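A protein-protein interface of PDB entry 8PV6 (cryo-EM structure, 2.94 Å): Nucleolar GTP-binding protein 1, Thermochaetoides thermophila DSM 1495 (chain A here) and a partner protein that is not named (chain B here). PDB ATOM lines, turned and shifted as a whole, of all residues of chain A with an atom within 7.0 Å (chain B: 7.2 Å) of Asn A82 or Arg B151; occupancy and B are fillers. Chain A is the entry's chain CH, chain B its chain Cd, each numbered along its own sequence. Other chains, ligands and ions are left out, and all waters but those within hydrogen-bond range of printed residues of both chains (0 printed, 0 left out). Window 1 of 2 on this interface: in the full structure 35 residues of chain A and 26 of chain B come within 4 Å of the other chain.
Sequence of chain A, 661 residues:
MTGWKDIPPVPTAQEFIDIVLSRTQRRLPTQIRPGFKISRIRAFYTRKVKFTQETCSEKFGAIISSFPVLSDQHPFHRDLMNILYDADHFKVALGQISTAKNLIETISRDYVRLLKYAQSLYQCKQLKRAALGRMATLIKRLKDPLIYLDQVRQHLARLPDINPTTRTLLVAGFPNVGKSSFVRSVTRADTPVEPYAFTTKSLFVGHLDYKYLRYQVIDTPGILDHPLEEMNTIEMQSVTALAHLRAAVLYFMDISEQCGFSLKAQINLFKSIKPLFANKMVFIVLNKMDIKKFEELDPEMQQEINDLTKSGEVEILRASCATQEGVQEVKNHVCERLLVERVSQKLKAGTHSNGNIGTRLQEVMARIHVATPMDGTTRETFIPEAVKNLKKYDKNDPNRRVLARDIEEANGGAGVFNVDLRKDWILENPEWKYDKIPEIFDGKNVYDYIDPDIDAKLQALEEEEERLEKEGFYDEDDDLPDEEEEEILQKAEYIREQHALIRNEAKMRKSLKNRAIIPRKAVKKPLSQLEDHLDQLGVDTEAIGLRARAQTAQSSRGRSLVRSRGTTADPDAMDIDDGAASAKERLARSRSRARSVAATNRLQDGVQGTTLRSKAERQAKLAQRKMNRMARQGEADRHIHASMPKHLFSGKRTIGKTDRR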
ATOM      1  N   LEU A  70      15.741  -2.601 -19.898  1.00  0.00           N
ATOM      2  CA  LEU A  70      15.975  -2.980 -21.292  1.00  0.00           C
ATOM      3  C   LEU A  70      15.379  -1.975 -22.267  1.00  0.00           C
ATOM      4  O   LEU A  70      15.936  -1.741 -23.347  1.00  0.00           O
ATOM      5  CB  LEU A  70      15.406  -4.373 -21.560  1.00  0.00           C
ATOM      6  CG  LEU A  70      16.393  -5.541 -21.560  1.00  0.00           C
ATOM      7  CD1 LEU A  70      16.977  -5.753 -20.183  1.00  0.00           C
ATOM      8  CD2 LEU A  70      15.714  -6.805 -22.053  1.00  0.00           C
ATOM      9  N   PHE A  76      21.694  -2.357 -29.358  1.00  0.00           N
ATOM     10  CA  PHE A  76      22.745  -3.366 -29.275  1.00  0.00           C
ATOM     11  C   PHE A  76      22.788  -4.003 -27.894  1.00  0.00           C
ATOM     12  O   PHE A  76      22.838  -5.229 -27.772  1.00  0.00           O
ATOM     13  CB  PHE A  76      24.102  -2.752 -29.616  1.00  0.00           C
ATOM     14  CG  PHE A  76      25.268  -3.619 -29.235  1.00  0.00           C
ATOM     15  CD1 PHE A  76      25.531  -4.787 -29.929  1.00  0.00           C
ATOM     16  CD2 PHE A  76      26.094  -3.271 -28.181  1.00  0.00           C
ATOM     17  CE1 PHE A  76      26.598  -5.590 -29.578  1.00  0.00           C
ATOM     18  CE2 PHE A  76      27.163  -4.071 -27.827  1.00  0.00           C
ATOM     19  CZ  PHE A  76      27.415  -5.231 -28.527  1.00  0.00           C
ATOM     20  N   HIS A  77      22.765  -3.183 -26.841  1.00  0.00           N
ATOM     21  CA  HIS A  77      22.807  -3.716 -25.483  1.00  0.00           C
ATOM     22  C   HIS A  77      21.539  -4.489 -25.149  1.00  0.00           C
ATOM     23  O   HIS A  77      21.599  -5.549 -24.514  1.00  0.00           O
ATOM     24  CB  HIS A  77      23.024  -2.587 -24.478  1.00  0.00           C
ATOM     25  CG  HIS A  77      24.407  -2.015 -24.502  1.00  0.00           C
ATOM     26  ND1 HIS A  77      25.518  -2.749 -24.150  1.00  0.00           N
ATOM     27  CD2 HIS A  77      24.857  -0.782 -24.829  1.00  0.00           C
ATOM     28  CE1 HIS A  77      26.596  -1.993 -24.263  1.00  0.00           C
ATOM     29  NE2 HIS A  77      26.221  -0.794 -24.673  1.00  0.00           N
ATOM     30  N   ARG A  78      20.382  -3.979 -25.581  1.00  0.00           N
ATOM     31  CA  ARG A  78      19.115  -4.660 -25.331  1.00  0.00           C
ATOM     32  C   ARG A  78      19.070  -6.023 -26.011  1.00  0.00           C
ATOM     33  O   ARG A  78      18.714  -7.029 -25.383  1.00  0.00           O
ATOM     34  CB  ARG A  78      17.957  -3.787 -25.811  1.00  0.00           C
ATOM     35  CG  ARG A  78      16.598  -4.450 -25.726  1.00  0.00           C
ATOM     36  CD  ARG A  78      15.491  -3.480 -26.122  1.00  0.00           C
ATOM     37  NE  ARG A  78      15.742  -2.835 -27.407  1.00  0.00           N
ATOM     38  CZ  ARG A  78      15.628  -3.425 -28.590  1.00  0.00           C
ATOM     39  NH1 ARG A  78      15.224  -4.680 -28.705  1.00  0.00           N
ATOM     40  NH2 ARG A  78      15.920  -2.735 -29.689  1.00  0.00           N
ATOM     41  N   ASP A  79      19.476  -6.092 -27.279  1.00  0.00           N
ATOM     42  CA  ASP A  79      19.439  -7.370 -27.978  1.00  0.00           C
ATOM     43  C   ASP A  79      20.561  -8.298 -27.522  1.00  0.00           C
ATOM     44  O   ASP A  79      20.395  -9.521 -27.544  1.00  0.00           O
ATOM     45  CB  ASP A  79      19.485  -7.136 -29.485  1.00  0.00           C
ATOM     46  CG  ASP A  79      18.212  -6.495 -30.003  1.00  0.00           C
ATOM     47  OD1 ASP A  79      17.146  -6.726 -29.398  1.00  0.00           O
ATOM     48  OD2 ASP A  79      18.272  -5.750 -31.001  1.00  0.00           O
ATOM     49  N   LEU A  80      21.693  -7.749 -27.074  1.00  0.00           N
ATOM     50  CA  LEU A  80      22.749  -8.585 -26.512  1.00  0.00           C
ATOM     51  C   LEU A  80      22.307  -9.222 -25.203  1.00  0.00           C
ATOM     52  O   LEU A  80      22.591 -10.400 -24.950  1.00  0.00           O
ATOM     53  CB  LEU A  80      24.017  -7.757 -26.303  1.00  0.00           C
ATOM     54  CG  LEU A  80      25.206  -8.495 -25.688  1.00  0.00           C
ATOM     55  CD1 LEU A  80      25.607  -9.674 -26.553  1.00  0.00           C
ATOM     56  CD2 LEU A  80      26.375  -7.551 -25.485  1.00  0.00           C
ATOM     57  N   MET A  81      21.605  -8.463 -24.359  1.00  0.00           N
ATOM     58  CA  MET A  81      21.061  -9.053 -23.141  1.00  0.00           C
ATOM     59  C   MET A  81      19.927 -10.017 -23.459  1.00  0.00           C
ATOM     60  O   MET A  81      19.692 -10.966 -22.707  1.00  0.00           O
ATOM     61  CB  MET A  81      20.593  -7.962 -22.178  1.00  0.00           C
ATOM     62  CG  MET A  81      21.716  -7.107 -21.618  1.00  0.00           C
ATOM     63  SD  MET A  81      21.126  -5.883 -20.437  1.00  0.00           S
ATOM     64  CE  MET A  81      20.345  -4.708 -21.533  1.00  0.00           C
ATOM     65  N   ASN A  82      19.223  -9.798 -24.571  1.00  0.00           N
ATOM     66  CA  ASN A  82      18.207 -10.754 -25.005  1.00  0.00           C
ATOM     67  C   ASN A  82      18.841 -12.059 -25.479  1.00  0.00           C
ATOM     68  O   ASN A  82      18.240 -13.134 -25.372  1.00  0.00           O
ATOM     69  CB  ASN A  82      17.351 -10.138 -26.111  1.00  0.00           C
ATOM     70  CG  ASN A  82      16.283 -11.084 -26.619  1.00  0.00           C
ATOM     71  OD1 ASN A  82      15.693 -11.844 -25.852  1.00  0.00           O
ATOM     72  ND2 ASN A  82      16.035 -11.048 -27.923  1.00  0.00           N
ATOM     73  N   ILE A  83      20.042 -11.979 -26.052  1.00  0.00           N
ATOM     74  CA  ILE A  83      20.749 -13.195 -26.451  1.00  0.00           C
ATOM     75  C   ILE A  83      21.301 -13.920 -25.229  1.00  0.00           C
ATOM     76  O   ILE A  83      21.117 -15.133 -25.071  1.00  0.00           O
ATOM     77  CB  ILE A  83      21.860 -12.867 -27.465  1.00  0.00           C
ATOM     78  CG1 ILE A  83      21.249 -12.360 -28.770  1.00  0.00           C
ATOM     79  CG2 ILE A  83      22.727 -14.084 -27.724  1.00  0.00           C
ATOM     80  CD1 ILE A  83      20.228 -13.297 -29.364  1.00  0.00           C
ATOM     81  N   LEU A  84      21.982 -13.186 -24.345  1.00  0.00           N
ATOM     82  CA  LEU A  84      22.635 -13.805 -23.194  1.00  0.00           C
ATOM     83  C   LEU A  84      21.620 -14.361 -22.203  1.00  0.00           C
ATOM     84  O   LEU A  84      21.781 -15.472 -21.685  1.00  0.00           O
ATOM     85  CB  LEU A  84      23.550 -12.795 -22.501  1.00  0.00           C
ATOM     86  CG  LEU A  84      24.779 -12.314 -23.265  1.00  0.00           C
ATOM     87  CD1 LEU A  84      25.396 -11.115 -22.576  1.00  0.00           C
ATOM     88  CD2 LEU A  84      25.785 -13.438 -23.368  1.00  0.00           C
ATOM     89  N   TYR A  85      20.567 -13.598 -21.927  1.00  0.00           N
ATOM     90  CA  TYR A  85      19.565 -13.942 -20.931  1.00  0.00           C
ATOM     91  C   TYR A  85      18.236 -13.976 -21.661  1.00  0.00           C
ATOM     92  O   TYR A  85      18.039 -13.210 -22.607  1.00  0.00           O
ATOM     93  CB  TYR A  85      19.510 -12.888 -19.824  1.00  0.00           C
ATOM     94  CG  TYR A  85      20.859 -12.423 -19.330  1.00  0.00           C
ATOM     95  CD1 TYR A  85      21.137 -11.066 -19.227  1.00  0.00           C
ATOM     96  CD2 TYR A  85      21.852 -13.324 -18.969  1.00  0.00           C
ATOM     97  CE1 TYR A  85      22.361 -10.618 -18.791  1.00  0.00           C
ATOM     98  CE2 TYR A  85      23.087 -12.882 -18.527  1.00  0.00           C
ATOM     99  CZ  TYR A  85      23.331 -11.527 -18.439  1.00  0.00           C
ATOM    100  OH  TYR A  85      24.548 -11.071 -18.000  1.00  0.00           O
ATOM    101  N   ASP A  86      17.325 -14.846 -21.247  1.00  0.00           N
ATOM    102  CA  ASP A  86      15.974 -14.741 -21.777  1.00  0.00           C
ATOM    103  C   ASP A  86      15.356 -13.447 -21.269  1.00  0.00           C
ATOM    104  O   ASP A  86      15.193 -13.264 -20.061  1.00  0.00           O
ATOM    105  CB  ASP A  86      15.133 -15.945 -21.357  1.00  0.00           C
ATOM    106  CG  ASP A  86      13.884 -16.107 -22.199  1.00  0.00           C
ATOM    107  OD1 ASP A  86      13.666 -15.287 -23.115  1.00  0.00           O
ATOM    108  OD2 ASP A  86      13.117 -17.060 -21.946  1.00  0.00           O
ATOM    109  N   ALA A  87      15.074 -12.527 -22.197  1.00  0.00           N
ATOM    110  CA  ALA A  87      14.565 -11.210 -21.820  1.00  0.00           C
ATOM    111  C   ALA A  87      13.210 -11.319 -21.137  1.00  0.00           C
ATOM    112  O   ALA A  87      12.907 -10.554 -20.210  1.00  0.00           O
ATOM    113  CB  ALA A  87      14.475 -10.309 -23.049  1.00  0.00           C
ATOM    114  N   ASP A  88      12.393 -12.279 -21.574  1.00  0.00           N
ATOM    115  CA  ASP A  88      11.139 -12.566 -20.891  1.00  0.00           C
ATOM    116  C   ASP A  88      11.387 -12.988 -19.451  1.00  0.00           C
ATOM    117  O   ASP A  88      10.729 -12.493 -18.534  1.00  0.00           O
ATOM    118  CB  ASP A  88      10.369 -13.650 -21.645  1.00  0.00           C
ATOM    119  CG  ASP A  88      10.153 -13.302 -23.101  1.00  0.00           C
ATOM    120  OD1 ASP A  88      10.281 -12.113 -23.457  1.00  0.00           O
ATOM    121  OD2 ASP A  88       9.854 -14.220 -23.894  1.00  0.00           O
ATOM    122  N   HIS A  89      12.360 -13.876 -19.229  1.00  0.00           N
ATOM    123  CA  HIS A  89      12.653 -14.343 -17.874  1.00  0.00           C
ATOM    124  C   HIS A  89      13.220 -13.224 -17.009  1.00  0.00           C
ATOM    125  O   HIS A  89      12.924 -13.141 -15.813  1.00  0.00           O
ATOM    126  CB  HIS A  89      13.622 -15.520 -17.930  1.00  0.00           C
ATOM    127  CG  HIS A  89      12.954 -16.838 -18.163  1.00  0.00           C
ATOM    128  ND1 HIS A  89      12.484 -17.224 -19.398  1.00  0.00           N
ATOM    129  CD2 HIS A  89      12.682 -17.861 -17.320  1.00  0.00           C
ATOM    130  CE1 HIS A  89      11.947 -18.427 -19.305  1.00  0.00           C
ATOM    131  NE2 HIS A  89      12.054 -18.836 -18.055  1.00  0.00           N
ATOM    132  N   THR A 233      23.138 -19.256 -29.122  1.00  0.00           N
ATOM    133  CA  THR A 233      23.396 -17.957 -28.504  1.00  0.00           C
ATOM    134  C   THR A 233      24.820 -17.470 -28.743  1.00  0.00           C
ATOM    135  O   THR A 233      25.044 -16.259 -28.873  1.00  0.00           O
ATOM    136  CB  THR A 233      23.118 -18.030 -27.003  1.00  0.00           C
ATOM    137  OG1 THR A 233      23.978 -19.005 -26.405  1.00  0.00           O
ATOM    138  CG2 THR A 233      21.676 -18.424 -26.751  1.00  0.00           C
ATOM    139  N   GLU B 139       9.739 -22.937 -19.186  1.00  0.00           N
ATOM    140  CA  GLU B 139      11.189 -22.826 -19.029  1.00  0.00           C
ATOM    141  C   GLU B 139      11.497 -22.317 -17.628  1.00  0.00           C
ATOM    142  O   GLU B 139      11.201 -21.151 -17.312  1.00  0.00           O
ATOM    143  CB  GLU B 139      11.805 -21.903 -20.077  1.00  0.00           C
ATOM    144  CG  GLU B 139      11.288 -22.090 -21.493  1.00  0.00           C
ATOM    145  CD  GLU B 139      11.820 -21.041 -22.449  1.00  0.00           C
ATOM    146  OE1 GLU B 139      12.694 -20.248 -22.040  1.00  0.00           O
ATOM    147  OE2 GLU B 139      11.362 -21.007 -23.610  1.00  0.00           O
ATOM    148  N   SER B 142      16.316 -22.037 -13.689  1.00  0.00           N
ATOM    149  CA  SER B 142      17.560 -22.800 -13.649  1.00  0.00           C
ATOM    150  C   SER B 142      17.965 -23.279 -15.036  1.00  0.00           C
ATOM    151  O   SER B 142      19.157 -23.352 -15.351  1.00  0.00           O
ATOM    152  CB  SER B 142      17.417 -23.984 -12.695  1.00  0.00           C
ATOM    153  OG  SER B 142      18.560 -24.818 -12.750  1.00  0.00           O
ATOM    154  N   GLU B 143      16.987 -23.615 -15.879  1.00  0.00           N
ATOM    155  CA  GLU B 143      17.293 -24.056 -17.234  1.00  0.00           C
ATOM    156  C   GLU B 143      17.572 -22.892 -18.173  1.00  0.00           C
ATOM    157  O   GLU B 143      18.048 -23.115 -19.290  1.00  0.00           O
ATOM    158  CB  GLU B 143      16.145 -24.902 -17.783  1.00  0.00           C
ATOM    159  CG  GLU B 143      15.847 -26.142 -16.964  1.00  0.00           C
ATOM    160  CD  GLU B 143      14.770 -27.006 -17.589  1.00  0.00           C
ATOM    161  OE1 GLU B 143      14.354 -26.705 -18.728  1.00  0.00           O
ATOM    162  OE2 GLU B 143      14.341 -27.984 -16.944  1.00  0.00           O
ATOM    163  N   THR B 144      17.281 -21.662 -17.753  1.00  0.00           N
ATOM    164  CA  THR B 144      17.535 -20.505 -18.603  1.00  0.00           C
ATOM    165  C   THR B 144      18.980 -20.033 -18.493  1.00  0.00           C
ATOM    166  O   THR B 144      19.724 -20.038 -19.479  1.00  0.00           O
ATOM    167  CB  THR B 144      16.577 -19.371 -18.241  1.00  0.00           C
ATOM    168  OG1 THR B 144      15.227 -19.792 -18.467  1.00  0.00           O
ATOM    169  CG2 THR B 144      16.879 -18.149 -19.074  1.00  0.00           C
ATOM    170  N   PHE B 145      19.392 -19.616 -17.300  1.00  0.00           N
ATOM    171  CA  PHE B 145      20.731 -19.100 -17.070  1.00  0.00           C
ATOM    172  C   PHE B 145      21.250 -19.638 -15.747  1.00  0.00           C
ATOM    173  O   PHE B 145      20.505 -19.721 -14.767  1.00  0.00           O
ATOM    174  CB  PHE B 145      20.742 -17.568 -17.063  1.00  0.00           C
ATOM    175  CG  PHE B 145      22.116 -16.969 -17.053  1.00  0.00           C
ATOM    176  CD1 PHE B 145      22.655 -16.460 -15.886  1.00  0.00           C
ATOM    177  CD2 PHE B 145      22.866 -16.907 -18.213  1.00  0.00           C
ATOM    178  CE1 PHE B 145      23.919 -15.907 -15.874  1.00  0.00           C
ATOM    179  CE2 PHE B 145      24.130 -16.354 -18.208  1.00  0.00           C
ATOM    180  CZ  PHE B 145      24.656 -15.853 -17.035  1.00  0.00           C
ATOM    181  N   LYS B 148      23.584 -24.832 -14.382  1.00  0.00           N
ATOM    182  CA  LYS B 148      22.848 -25.984 -14.884  1.00  0.00           C
ATOM    183  C   LYS B 148      21.955 -25.621 -16.064  1.00  0.00           C
ATOM    184  O   LYS B 148      21.016 -26.360 -16.376  1.00  0.00           O
ATOM    185  CB  LYS B 148      22.014 -26.608 -13.764  1.00  0.00           C
ATOM    186  CG  LYS B 148      22.800 -26.912 -12.501  1.00  0.00           C
ATOM    187  CD  LYS B 148      23.872 -27.957 -12.744  1.00  0.00           C
ATOM    188  CE  LYS B 148      24.647 -28.250 -11.471  1.00  0.00           C
ATOM    189  NZ  LYS B 148      25.749 -29.223 -11.707  1.00  0.00           N
ATOM    190  N   ALA B 149      22.227 -24.494 -16.718  1.00  0.00           N
ATOM    191  CA  ALA B 149      21.358 -24.003 -17.777  1.00  0.00           C
ATOM    192  C   ALA B 149      21.437 -24.894 -19.012  1.00  0.00           C
ATOM    193  O   ALA B 149      22.511 -25.342 -19.419  1.00  0.00           O
ATOM    194  CB  ALA B 149      21.732 -22.570 -18.149  1.00  0.00           C
ATOM    195  N   GLN B 150      20.273 -25.148 -19.606  1.00  0.00           N
ATOM    196  CA  GLN B 150      20.173 -25.921 -20.834  1.00  0.00           C
ATOM    197  C   GLN B 150      19.639 -25.106 -22.000  1.00  0.00           C
ATOM    198  O   GLN B 150      19.388 -25.674 -23.069  1.00  0.00           O
ATOM    199  CB  GLN B 150      19.286 -27.155 -20.616  1.00  0.00           C
ATOM    200  CG  GLN B 150      19.620 -27.942 -19.359  1.00  0.00           C
ATOM    201  CD  GLN B 150      20.982 -28.608 -19.425  1.00  0.00           C
ATOM    202  OE1 GLN B 150      21.471 -28.948 -20.501  1.00  0.00           O
ATOM    203  NE2 GLN B 150      21.603 -28.791 -18.267  1.00  0.00           N
ATOM    204  N   ARG B 151      19.454 -23.800 -21.826  1.00  0.00           N
ATOM    205  CA  ARG B 151      18.963 -22.952 -22.903  1.00  0.00           C
ATOM    206  C   ARG B 151      20.037 -22.784 -23.970  1.00  0.00           C
ATOM    207  O   ARG B 151      21.184 -22.446 -23.664  1.00  0.00           O
ATOM    208  CB  ARG B 151      18.550 -21.590 -22.349  1.00  0.00           C
ATOM    209  CG  ARG B 151      18.339 -20.516 -23.402  1.00  0.00           C
ATOM    210  CD  ARG B 151      17.919 -19.205 -22.767  1.00  0.00           C
ATOM    211  NE  ARG B 151      17.729 -18.151 -23.756  1.00  0.00           N
ATOM    212  CZ  ARG B 151      18.660 -17.276 -24.104  1.00  0.00           C
ATOM    213  NH1 ARG B 151      19.870 -17.304 -23.570  1.00  0.00           N
ATOM    214  NH2 ARG B 151      18.372 -16.346 -25.010  1.00  0.00           N
ATOM    215  N   LYS B 152      19.661 -23.021 -25.227  1.00  0.00           N
ATOM    216  CA  LYS B 152      20.586 -22.885 -26.340  1.00  0.00           C
ATOM    217  C   LYS B 152      20.054 -22.041 -27.487  1.00  0.00           C
ATOM    218  O   LYS B 152      20.861 -21.500 -28.247  1.00  0.00           O
ATOM    219  CB  LYS B 152      20.975 -24.268 -26.887  1.00  0.00           C
ATOM    220  CG  LYS B 152      21.900 -25.057 -25.980  1.00  0.00           C
ATOM    221  CD  LYS B 152      23.354 -24.700 -26.221  1.00  0.00           C
ATOM    222  CE  LYS B 152      24.279 -25.622 -25.447  1.00  0.00           C
ATOM    223  NZ  LYS B 152      25.711 -25.287 -25.675  1.00  0.00           N
ATOM    224  N   ARG B 153      18.739 -21.902 -27.636  1.00  0.00           N
ATOM    225  CA  ARG B 153      18.156 -21.158 -28.744  1.00  0.00           C
ATOM    226  C   ARG B 153      17.459 -19.914 -28.213  1.00  0.00           C
ATOM    227  O   ARG B 153      16.484 -20.036 -27.450  1.00  0.00           O
ATOM    228  CB  ARG B 153      17.169 -22.029 -29.525  1.00  0.00           C
ATOM    229  CG  ARG B 153      17.678 -22.470 -30.884  1.00  0.00           C
ATOM    230  CD  ARG B 153      18.880 -23.384 -30.735  1.00  0.00           C
ATOM    231  NE  ARG B 153      19.277 -23.986 -32.001  1.00  0.00           N
ATOM    232  CZ  ARG B 153      20.297 -24.821 -32.144  1.00  0.00           C
ATOM    233  NH1 ARG B 153      21.048 -25.177 -31.115  1.00  0.00           N
ATOM    234  NH2 ARG B 153      20.570 -25.311 -33.350  1.00  0.00           N
ATOM    235  N   PRO B 154      17.906 -18.714 -28.572  1.00  0.00           N
ATOM    236  CA  PRO B 154      17.240 -17.502 -28.089  1.00  0.00           C
ATOM    237  C   PRO B 154      15.896 -17.290 -28.765  1.00  0.00           C
ATOM    238  O   PRO B 154      15.615 -17.813 -29.846  1.00  0.00           O
ATOM    239  CB  PRO B 154      18.227 -16.391 -28.457  1.00  0.00           C
ATOM    240  CG  PRO B 154      18.948 -16.924 -29.642  1.00  0.00           C
ATOM    241  CD  PRO B 154      19.064 -18.407 -29.427  1.00  0.00           C
ATOM    242  N   LYS B 155      15.053 -16.503 -28.101  1.00  0.00           N
ATOM    243  CA  LYS B 155      13.730 -16.148 -28.610  1.00  0.00           C
ATOM    244  C   LYS B 155      13.857 -14.813 -29.335  1.00  0.00           C
ATOM    245  O   LYS B 155      14.149 -13.784 -28.720  1.00  0.00           O
ATOM    246  CB  LYS B 155      12.712 -16.082 -27.479  1.00  0.00           C
ATOM    247  CG  LYS B 155      11.280 -15.885 -27.943  1.00  0.00           C
ATOM    248  CD  LYS B 155      10.323 -15.861 -26.764  1.00  0.00           C
ATOM    249  CE  LYS B 155      10.183 -17.238 -26.137  1.00  0.00           C
ATOM    250  NZ  LYS B 155       9.520 -18.204 -27.054  1.00  0.00           N
ATOM    251  N   LEU B 156      13.640 -14.833 -30.644  1.00  0.00           N
ATOM    252  CA  LEU B 156      13.854 -13.671 -31.492  1.00  0.00           C
ATOM    253  C   LEU B 156      12.547 -13.187 -32.107  1.00  0.00           C
ATOM    254  O   LEU B 156      11.587 -13.945 -32.270  1.00  0.00           O
ATOM    255  CB  LEU B 156      14.861 -13.996 -32.595  1.00  0.00           C
ATOM    256  CG  LEU B 156      16.051 -14.836 -32.134  1.00  0.00           C
ATOM    257  CD1 LEU B 156      16.812 -15.383 -33.322  1.00  0.00           C
ATOM    258  CD2 LEU B 156      16.959 -14.016 -31.236  1.00  0.00           C
ATOM    259  N   SER B 157      12.525 -11.900 -32.451  1.00  0.00           N
ATOM    260  CA  SER B 157      11.390 -11.273 -33.113  1.00  0.00           C
ATOM    261  C   SER B 157      11.614 -11.106 -34.610  1.00  0.00           C
ATOM    262  O   SER B 157      10.826 -10.430 -35.279  1.00  0.00           O
ATOM    263  CB  SER B 157      11.086  -9.919 -32.473  1.00  0.00           C
ATOM    264  OG  SER B 157      10.908 -10.054 -31.077  1.00  0.00           O
ATOM    265  N   PHE B 158      12.669 -11.709 -35.146  1.00  0.00           N
ATOM    266  CA  PHE B 158      12.996 -11.629 -36.560  1.00  0.00           C
ATOM    267  C   PHE B 158      13.307 -13.026 -37.068  1.00  0.00           C
ATOM    268  O   PHE B 158      13.735 -13.890 -36.298  1.00  0.00           O
ATOM    269  CB  PHE B 158      14.178 -10.679 -36.808  1.00  0.00           C
ATOM    270  CG  PHE B 158      15.359 -10.925 -35.906  1.00  0.00           C
ATOM    271  CD1 PHE B 158      15.487 -10.237 -34.708  1.00  0.00           C
ATOM    272  CD2 PHE B 158      16.349 -11.828 -36.259  1.00  0.00           C
ATOM    273  CE1 PHE B 158      16.569 -10.456 -33.875  1.00  0.00           C
ATOM    274  CE2 PHE B 158      17.434 -12.049 -35.429  1.00  0.00           C
ATOM    275  CZ  PHE B 158      17.543 -11.363 -34.236  1.00  0.00           C
ATOM    276  N   TYR B 167      14.541  -4.575 -38.409  1.00  0.00           N
ATOM    277  CA  TYR B 167      14.324  -4.499 -36.969  1.00  0.00           C
ATOM    278  C   TYR B 167      15.359  -3.603 -36.305  1.00  0.00           C
ATOM    279  O   TYR B 167      15.018  -2.765 -35.464  1.00  0.00           O
ATOM    280  CB  TYR B 167      14.363  -5.915 -36.387  1.00  0.00           C
ATOM    281  CG  TYR B 167      14.491  -6.006 -34.884  1.00  0.00           C
ATOM    282  CD1 TYR B 167      15.540  -6.708 -34.305  1.00  0.00           C
ATOM    283  CD2 TYR B 167      13.552  -5.424 -34.046  1.00  0.00           C
ATOM    284  CE1 TYR B 167      15.662  -6.808 -32.932  1.00  0.00           C
ATOM    285  CE2 TYR B 167      13.666  -5.516 -32.668  1.00  0.00           C
ATOM    286  CZ  TYR B 167      14.723  -6.210 -32.118  1.00  0.00           C
ATOM    287  OH  TYR B 167      14.844  -6.309 -30.751  1.00  0.00           O
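The backbone carbonyl oxygen (O) of Glu B139 is in hydrogen-bond range of a ring nitrogen (NE2) of His A89 (2.6 Å).
A ring nitrogen (NE2) of His A89 is in hydrogen-bond range of the side-chain hydroxyl (OG1) of Thr B144 (3.3 Å).
The guanidinium group of Arg B151 lies within hydrogen-bond range of the backbone carbonyl oxygen of Asn A82 (3.2 Å).
O of Ile A83 sits at hydrogen-bond distance from NH1 of Arg B151 (2.9 Å).
NH1 of Arg B151 sits at hydrogen-bond distance from O of Leu A84 (3.2 Å).
The backbone carbonyl oxygen (O) of Lys B152 lies within hydrogen-bond range of the backbone NH (N) of Thr A233, at 3.3 Å.
O of Lys B155 lies within hydrogen-bond range of ND2 of Asn A82, at 3.4 Å.
The side-chain hydroxyl (OH) of Tyr B167 sits at hydrogen-bond distance from the guanidinium group (NH1) of Arg A78 (2.6 Å).
OH of Tyr B167 is in hydrogen-bond range of OD1 of Asp A79, at 2.7 Å.
The side-chain carboxylate (OE1) of Glu B139 lies close to the side-chain carboxylate (OD2) of Asp A86 (3.2 Å).
The backbone carbonyl oxygen (O) of Glu B143 sits at hydrogen-bond distance from the backbone NH (N) of Arg B151.
OD1 of Asp A79 is in salt-bridge range of NH1 of Arg A78, 2.9 Å away.
The side-chain carboxylate of Asp A86 lies within hydrogen-bond range of a ring nitrogen (ND1) of His A89, 2.6 Å away.
Among the printed residues, pairs that only touch across the chains: Asp A88 with Lys B155 (3.3 Å), Asp A86 with Thr B144 (3.6 Å), Tyr A85 with Phe B145 (3.6 Å), Thr A233 with Pro B154 (3.7 Å), Ile A83 with Pro B154 (3.8 Å), Thr A233 with Arg B151 (3.8 Å), Ile A83 with Leu B156 (3.8 Å), Leu A84 with Phe B145 (3.9 Å), Tyr A85 with Arg B151 (3.96 Å) and Asp A86 with Arg B151 (3.98 Å).
Of chain B, only Arg B151 and Lys B155 come within 4 Å of Asn A82.
Of the printed residues of chain A, Arg B151 touches Asn A82 (3.2 Å), Ile A83 (2.9 Å), Leu A84 (3.2 Å), Tyr A85 (3.96 Å), Asp A86 (3.98 Å) and Thr A233 (3.8 Å).
Printed residues of chain A within 4 Å of Tyr B167: Arg A78 and Asp A79.
Of the printed residues of chain A, Glu B139 touches Asp A86 and His A89.
Printed residues of chain B within 4 Å of Asp A88: Lys B155.
Leu A70 touches none of the printed residues of chain B.
The nearest residue of chain B that does not touch Asn A82 is Pro B154 (4.5 Å).
The nearest printed residue of chain A that does not touch Arg B151 is Ala A87 (5.8 Å).
The nearest printed residue of chain B that does not touch Asp A86 is Lys B155 (4.5 Å).
Of the 17 printed residues of chain B, 9 touch a printed residue of chain A.
Hydrophobic or aromatic side chains of chain B within 4 Å of the printed part of chain A: Phe B145, Pro B154, Leu B156 and Tyr B167.
Along chain A the printed residues that touch a printed residue of chain B span positions 78 to 233.
Among the printed residues, 20 pairs touch across the chains.
Among the printed residues, no Asp or Glu carboxylate lies within 4 Å of a Lys or Arg side-chain nitrogen of the other chain.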
